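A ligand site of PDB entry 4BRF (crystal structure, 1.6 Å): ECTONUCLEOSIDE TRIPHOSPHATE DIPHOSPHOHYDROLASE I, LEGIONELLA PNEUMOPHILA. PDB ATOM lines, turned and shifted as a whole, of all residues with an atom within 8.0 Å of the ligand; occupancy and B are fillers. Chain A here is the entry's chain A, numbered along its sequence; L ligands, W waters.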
ATOM      1  N   ASP A  63      -2.982 -31.771  23.661  1.00  0.00           N
ATOM      2  CA  ASP A  63      -3.209 -31.763  22.214  1.00  0.00           C
ATOM      3  C   ASP A  63      -4.004 -30.507  21.802  1.00  0.00           C
ATOM      4  O   ASP A  63      -3.632 -29.815  20.838  1.00  0.00           O
ATOM      5  CB  ASP A  63      -3.952 -33.028  21.697  1.00  0.00           C
ATOM      6  CG  ASP A  63      -4.404 -32.872  20.228  1.00  0.00           C
ATOM      7  OD1 ASP A  63      -3.541 -32.772  19.313  1.00  0.00           O
ATOM      8  OD2 ASP A  63      -5.623 -32.828  19.980  1.00  0.00           O
ATOM      9  N   LEU A  66      -1.589 -27.248  22.408  1.00  0.00           N
ATOM     10  CA  LEU A  66      -0.527 -27.157  21.371  1.00  0.00           C
ATOM     11  C   LEU A  66      -1.091 -26.963  19.934  1.00  0.00           C
ATOM     12  O   LEU A  66      -0.550 -26.161  19.172  1.00  0.00           O
ATOM     13  CB  LEU A  66       0.448 -28.319  21.472  1.00  0.00           C
ATOM     14  CG  LEU A  66       1.188 -28.418  22.825  1.00  0.00           C
ATOM     15  CD1 LEU A  66       2.001 -29.708  22.928  1.00  0.00           C
ATOM     16  CD2 LEU A  66       2.053 -27.158  23.100  1.00  0.00           C
ATOM     17  N   THR A  67      -2.196 -27.668  19.576  1.00  0.00           N
ATOM     18  CA  THR A  67      -2.830 -27.431  18.282  1.00  0.00           C
ATOM     19  C   THR A  67      -3.243 -25.950  18.163  1.00  0.00           C
ATOM     20  O   THR A  67      -2.965 -25.322  17.109  1.00  0.00           O
ATOM     21  CB  THR A  67      -4.061 -28.308  18.156  1.00  0.00           C
ATOM     22  OG1 THR A  67      -3.622 -29.677  18.046  1.00  0.00           O
ATOM     23  CG2 THR A  67      -4.947 -27.899  16.950  1.00  0.00           C
ATOM     24  N   MET A  68      -3.900 -25.406  19.214  1.00  0.00           N
ATOM     25  CA  MET A  68      -4.357 -24.024  19.167  1.00  0.00           C
ATOM     26  C   MET A  68      -3.149 -23.054  19.052  1.00  0.00           C
ATOM     27  O   MET A  68      -3.230 -21.977  18.382  1.00  0.00           O
ATOM     28  CB  MET A  68      -5.160 -23.633  20.416  1.00  0.00           C
ATOM     29  CG  MET A  68      -6.047 -22.359  20.244  1.00  0.00           C
ATOM     30  SD  MET A  68      -6.971 -22.000  21.751  1.00  0.00           S
ATOM     31  CE  MET A  68      -8.282 -23.176  21.420  1.00  0.00           C
ATOM     32  N   LEU A  69      -2.021 -23.416  19.666  1.00  0.00           N
ATOM     33  CA  LEU A  69      -0.857 -22.528  19.666  1.00  0.00           C
ATOM     34  C   LEU A  69      -0.151 -22.601  18.297  1.00  0.00           C
ATOM     35  O   LEU A  69       0.300 -21.580  17.767  1.00  0.00           O
ATOM     36  CB  LEU A  69       0.114 -22.977  20.761  1.00  0.00           C
ATOM     37  CG  LEU A  69       1.408 -22.155  20.844  1.00  0.00           C
ATOM     38  CD1 LEU A  69       1.076 -20.700  21.202  1.00  0.00           C
ATOM     39  CD2 LEU A  69       2.331 -22.785  21.868  1.00  0.00           C
ATOM     40  N   LEU A  70      -0.054 -23.813  17.730  1.00  0.00           N
ATOM     41  CA  LEU A  70       0.922 -24.067  16.636  1.00  0.00           C
ATOM     42  C   LEU A  70       0.344 -24.401  15.260  1.00  0.00           C
ATOM     43  O   LEU A  70       0.980 -24.163  14.230  1.00  0.00           O
ATOM     44  CB  LEU A  70       1.848 -25.249  17.033  1.00  0.00           C
ATOM     45  CG  LEU A  70       2.791 -25.048  18.246  1.00  0.00           C
ATOM     46  CD1 LEU A  70       3.289 -26.330  18.931  1.00  0.00           C
ATOM     47  CD2 LEU A  70       3.968 -24.165  17.868  1.00  0.00           C
ATOM     48  N   ALA A  71      -0.824 -25.042  15.225  1.00  0.00           N
ATOM     49  CA  ALA A  71      -1.303 -25.590  13.929  1.00  0.00           C
ATOM     50  C   ALA A  71      -1.423 -24.556  12.804  1.00  0.00           C
ATOM     51  O   ALA A  71      -1.128 -24.907  11.645  1.00  0.00           O
ATOM     52  CB  ALA A  71      -2.622 -26.389  14.080  1.00  0.00           C
ATOM     53  N   ASP A  72      -1.847 -23.308  13.078  1.00  0.00           N
ATOM     54  CA  ASP A  72      -2.013 -22.315  11.949  1.00  0.00           C
ATOM     55  C   ASP A  72      -0.769 -21.473  11.653  1.00  0.00           C
ATOM     56  O   ASP A  72      -0.835 -20.512  10.871  1.00  0.00           O
ATOM     57  CB  ASP A  72      -3.215 -21.394  12.163  1.00  0.00           C
ATOM     58  CG  ASP A  72      -3.089 -20.557  13.447  1.00  0.00           C
ATOM     59  OD1 ASP A  72      -2.018 -20.667  14.180  1.00  0.00           O
ATOM     60  OD2 ASP A  72      -4.047 -19.769  13.658  1.00  0.00           O
ATOM     61  N   ALA A  73       0.369 -21.813  12.261  1.00  0.00           N
ATOM     62  CA  ALA A  73       1.611 -21.106  11.959  1.00  0.00           C
ATOM     63  C   ALA A  73       1.914 -21.237  10.456  1.00  0.00           C
ATOM     64  O   ALA A  73       1.615 -22.294   9.821  1.00  0.00           O
ATOM     65  CB  ALA A  73       2.792 -21.646  12.781  1.00  0.00           C
ATOM     66  N   ILE A  75       4.753 -21.605   8.825  1.00  0.00           N
ATOM     67  CA  ILE A  75       5.974 -22.354   8.541  1.00  0.00           C
ATOM     68  C   ILE A  75       6.179 -23.335   9.731  1.00  0.00           C
ATOM     69  O   ILE A  75       6.222 -22.873  10.904  1.00  0.00           O
ATOM     70  CB  ILE A  75       7.201 -21.420   8.426  1.00  0.00           C
ATOM     71  CG1 ILE A  75       7.185 -20.575   7.118  1.00  0.00           C
ATOM     72  CG2 ILE A  75       8.478 -22.249   8.372  1.00  0.00           C
ATOM     73  CD1 ILE A  75       6.965 -19.076   7.299  1.00  0.00           C
ATOM     74  N   HIS A  76       6.290 -24.657   9.474  1.00  0.00           N
ATOM     75  CA  HIS A  76       6.377 -25.653  10.596  1.00  0.00           C
ATOM     76  C   HIS A  76       7.711 -26.424  10.633  1.00  0.00           C
ATOM     77  O   HIS A  76       8.048 -27.022  11.668  1.00  0.00           O
ATOM     78  CB  HIS A  76       5.182 -26.688  10.593  1.00  0.00           C
ATOM     79  CG  HIS A  76       3.800 -26.086  10.795  1.00  0.00           C
ATOM     80  ND1 HIS A  76       2.757 -26.797  11.355  1.00  0.00           N
ATOM     81  CD2 HIS A  76       3.288 -24.868  10.471  1.00  0.00           C
ATOM     82  CE1 HIS A  76       1.667 -26.045  11.390  1.00  0.00           C
ATOM     83  NE2 HIS A  76       1.965 -24.866  10.845  1.00  0.00           N
ATOM     84  N   ASN A  77       8.444 -26.442   9.503  1.00  0.00           N
ATOM     85  CA  ASN A  77       9.660 -27.307   9.349  1.00  0.00           C
ATOM     86  C   ASN A  77      10.920 -26.584   9.907  1.00  0.00           C
ATOM     87  O   ASN A  77      11.906 -26.338   9.149  1.00  0.00           O
ATOM     88  CB  ASN A  77       9.837 -27.823   7.899  1.00  0.00           C
ATOM     89  CG  ASN A  77      10.059 -26.706   6.899  1.00  0.00           C
ATOM     90  OD1 ASN A  77       9.486 -25.585   7.044  1.00  0.00           O
ATOM     91  ND2 ASN A  77      10.896 -26.984   5.875  1.00  0.00           N
ATOM     92  N   ILE A  78      10.871 -26.247  11.200  1.00  0.00           N
ATOM     93  CA  ILE A  78      11.901 -25.387  11.837  1.00  0.00           C
ATOM     94  C   ILE A  78      12.115 -25.863  13.260  1.00  0.00           C
ATOM     95  O   ILE A  78      11.220 -26.497  13.830  1.00  0.00           O
ATOM     96  CB  ILE A  78      11.491 -23.886  11.782  1.00  0.00           C
ATOM     97  CG1 ILE A  78      10.070 -23.656  12.427  1.00  0.00           C
ATOM     98  CG2 ILE A  78      11.485 -23.406  10.301  1.00  0.00           C
ATOM     99  CD1 ILE A  78       9.640 -22.162  12.501  1.00  0.00           C
ATOM    100  N   TRP A 106       3.384 -35.257  22.000  1.00  0.00           N
ATOM    101  CA  TRP A 106       2.638 -34.567  20.949  1.00  0.00           C
ATOM    102  C   TRP A 106       3.582 -34.211  19.834  1.00  0.00           C
ATOM    103  O   TRP A 106       3.279 -34.451  18.630  1.00  0.00           O
ATOM    104  CB  TRP A 106       2.050 -33.281  21.501  1.00  0.00           C
ATOM    105  CG  TRP A 106       1.151 -32.528  20.578  1.00  0.00           C
ATOM    106  CD1 TRP A 106      -0.205 -32.701  20.462  1.00  0.00           C
ATOM    107  CD2 TRP A 106       1.505 -31.450  19.663  1.00  0.00           C
ATOM    108  NE1 TRP A 106      -0.724 -31.816  19.533  1.00  0.00           N
ATOM    109  CE2 TRP A 106       0.285 -31.024  19.026  1.00  0.00           C
ATOM    110  CE3 TRP A 106       2.724 -30.821  19.307  1.00  0.00           C
ATOM    111  CZ2 TRP A 106       0.252 -29.969  18.046  1.00  0.00           C
ATOM    112  CZ3 TRP A 106       2.691 -29.725  18.341  1.00  0.00           C
ATOM    113  CH2 TRP A 106       1.444 -29.349  17.713  1.00  0.00           C
ATOM    114  N   PHE A 107       4.774 -33.683  20.201  1.00  0.00           N
ATOM    115  CA  PHE A 107       5.788 -33.368  19.158  1.00  0.00           C
ATOM    116  C   PHE A 107       6.214 -34.616  18.349  1.00  0.00           C
ATOM    117  O   PHE A 107       6.532 -34.522  17.162  1.00  0.00           O
ATOM    118  CB  PHE A 107       6.951 -32.532  19.697  1.00  0.00           C
ATOM    119  CG  PHE A 107       6.618 -31.069  19.819  1.00  0.00           C
ATOM    120  CD1 PHE A 107       6.798 -30.224  18.718  1.00  0.00           C
ATOM    121  CD2 PHE A 107       6.108 -30.516  21.037  1.00  0.00           C
ATOM    122  CE1 PHE A 107       6.506 -28.846  18.819  1.00  0.00           C
ATOM    123  CE2 PHE A 107       5.797 -29.144  21.123  1.00  0.00           C
ATOM    124  CZ  PHE A 107       5.971 -28.317  20.008  1.00  0.00           C
ATOM    125  N   GLN A 109       4.417 -36.901  17.295  1.00  0.00           N
ATOM    126  CA  GLN A 109       3.437 -37.189  16.229  1.00  0.00           C
ATOM    127  C   GLN A 109       3.391 -36.115  15.145  1.00  0.00           C
ATOM    128  O   GLN A 109       2.548 -36.190  14.266  1.00  0.00           O
ATOM    129  CB  GLN A 109       2.010 -37.344  16.810  1.00  0.00           C
ATOM    130  CG  GLN A 109       1.917 -38.026  18.175  1.00  0.00           C
ATOM    131  CD  GLN A 109       2.687 -39.331  18.236  1.00  0.00           C
ATOM    132  OE1 GLN A 109       3.463 -39.565  19.159  1.00  0.00           O
ATOM    133  NE2 GLN A 109       2.479 -40.188  17.272  1.00  0.00           N
ATOM    134  N   GLN A 110       4.243 -35.108  15.225  1.00  0.00           N
ATOM    135  CA  GLN A 110       4.364 -34.028  14.209  1.00  0.00           C
ATOM    136  C   GLN A 110       5.513 -34.424  13.280  1.00  0.00           C
ATOM    137  O   GLN A 110       6.603 -34.845  13.746  1.00  0.00           O
ATOM    138  CB  GLN A 110       4.654 -32.644  14.858  1.00  0.00           C
ATOM    139  CG  GLN A 110       3.593 -32.259  15.845  1.00  0.00           C
ATOM    140  CD  GLN A 110       2.335 -31.735  15.180  1.00  0.00           C
ATOM    141  OE1 GLN A 110       2.400 -30.938  14.233  1.00  0.00           O
ATOM    142  NE2 GLN A 110       1.178 -32.208  15.639  1.00  0.00           N
ATOM    143  N   SER A 111       5.307 -34.279  11.986  1.00  0.00           N
ATOM    144  CA  SER A 111       6.304 -34.689  11.054  1.00  0.00           C
ATOM    145  C   SER A 111       7.141 -33.472  10.578  1.00  0.00           C
ATOM    146  O   SER A 111       8.131 -33.686   9.852  1.00  0.00           O
ATOM    147  CB  SER A 111       5.640 -35.363   9.869  1.00  0.00           C
ATOM    148  OG  SER A 111       4.653 -34.468   9.386  1.00  0.00           O
ATOM    149  N   GLN A 112       6.785 -32.232  11.010  1.00  0.00           N
ATOM    150  CA  GLN A 112       7.454 -30.993  10.479  1.00  0.00           C
ATOM    151  C   GLN A 112       8.199 -30.252  11.608  1.00  0.00           C
ATOM    152  O   GLN A 112       9.428 -30.033  11.516  1.00  0.00           O
ATOM    153  CB  GLN A 112       6.469 -30.009   9.739  1.00  0.00           C
ATOM    154  CG  GLN A 112       5.827 -30.491   8.374  1.00  0.00           C
ATOM    155  CD  GLN A 112       6.811 -31.024   7.394  1.00  0.00           C
ATOM    156  OE1 GLN A 112       6.707 -32.173   6.976  1.00  0.00           O
ATOM    157  NE2 GLN A 112       7.773 -30.209   7.014  1.00  0.00           N
ATOM    158  N   TRP A 113       7.493 -29.908  12.687  1.00  0.00           N
ATOM    159  CA  TRP A 113       8.090 -29.190  13.822  1.00  0.00           C
ATOM    160  C   TRP A 113       9.292 -29.962  14.325  1.00  0.00           C
ATOM    161  O   TRP A 113       9.210 -31.250  14.451  1.00  0.00           O
ATOM    162  CB  TRP A 113       7.078 -29.055  14.978  1.00  0.00           C
ATOM    163  CG  TRP A 113       5.934 -28.107  14.713  1.00  0.00           C
ATOM    164  CD1 TRP A 113       4.600 -28.441  14.677  1.00  0.00           C
ATOM    165  CD2 TRP A 113       6.003 -26.692  14.485  1.00  0.00           C
ATOM    166  NE1 TRP A 113       3.834 -27.317  14.462  1.00  0.00           N
ATOM    167  CE2 TRP A 113       4.656 -26.233  14.328  1.00  0.00           C
ATOM    168  CE3 TRP A 113       7.073 -25.758  14.428  1.00  0.00           C
ATOM    169  CZ2 TRP A 113       4.327 -24.862  14.081  1.00  0.00           C
ATOM    170  CZ3 TRP A 113       6.765 -24.406  14.214  1.00  0.00           C
ATOM    171  CH2 TRP A 113       5.366 -23.955  14.025  1.00  0.00           C
ATOM    172  N   GLN A 114      10.409 -29.254  14.593  1.00  0.00           N
ATOM    173  CA  GLN A 114      11.621 -29.939  15.076  1.00  0.00           C
ATOM    174  C   GLN A 114      11.876 -29.481  16.550  1.00  0.00           C
ATOM    175  O   GLN A 114      12.558 -28.451  16.792  1.00  0.00           O
ATOM    176  CB  GLN A 114      12.806 -29.581  14.198  1.00  0.00           C
ATOM    177  CG  GLN A 114      12.580 -29.972  12.747  1.00  0.00           C
ATOM    178  CD  GLN A 114      13.500 -29.223  11.815  1.00  0.00           C
ATOM    179  OE1 GLN A 114      14.241 -28.312  12.251  1.00  0.00           O
ATOM    180  NE2 GLN A 114      13.446 -29.543  10.533  1.00  0.00           N
HETATM  181 MO1  LIG L   1       3.019 -30.911  11.540  1.00  0.00          MO
HETATM  182  O1  LIG L   1       3.188 -30.408   9.924  1.00  0.00           O
HETATM  183  O2  LIG L   1       4.636 -30.899  12.126  1.00  0.00           O
HETATM  184 MO2  LIG L   1       0.713 -29.481  13.270  1.00  0.00          MO
HETATM  185  O3  LIG L   1       2.447 -29.044  12.180  1.00  0.00           O
HETATM  186  O4  LIG L   1       1.063 -28.233  14.422  1.00  0.00           O
HETATM  187  O5  LIG L   1      -0.589 -30.268  14.075  1.00  0.00           O
HETATM  188  O6  LIG L   1      -0.376 -28.651  12.244  1.00  0.00           O
HETATM  189  O   HOH W   1      -2.717 -30.465  15.509  1.00  0.00           O
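A molybdenum atom (MO2) of the ligand is bound by the side-chain amide oxygen (OE1) of Gln 110 (2.4 Å). A ring nitrogen (ND1) of His 76 lies close to an oxygen (O3) of the ligand, 2.4 Å away.
The indole nitrogen (NE1) of Trp 106 lies within hydrogen-bond range of the side-chain carboxylate (OD1) of Asp 63 (3.0 Å). The backbone carbonyl oxygen (O) of His 76 sits close to the backbone NH (N) of Trp 113, 3.1 Å away. The backbone carbonyl oxygen (O) of Ala 71 lies close to a ring nitrogen (NE2) of His 76 (3.2 Å). The backbone carbonyl oxygen of Ala 73 lies within hydrogen-bond range of a ring nitrogen (NE2) of His 76 (2.8 Å).
N of Ser 111 lies close to O2 of the ligand (3.4 Å). The backbone NH (N) of Gln 112 lies close to an oxygen (O2) of the ligand, at 2.8 Å. The indole nitrogen (NE1) of Trp 113 lies close to an oxygen (O4) of the ligand (2.9 Å). Leu 70 touches the ligand (C to O4, 3.99 Å). Ala 71 touches the ligand. Trp 106 touches the ligand (CH2 to O4, 3.5 Å). Of the 21 residues printed, 8 come within 4 Å of the ligand.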
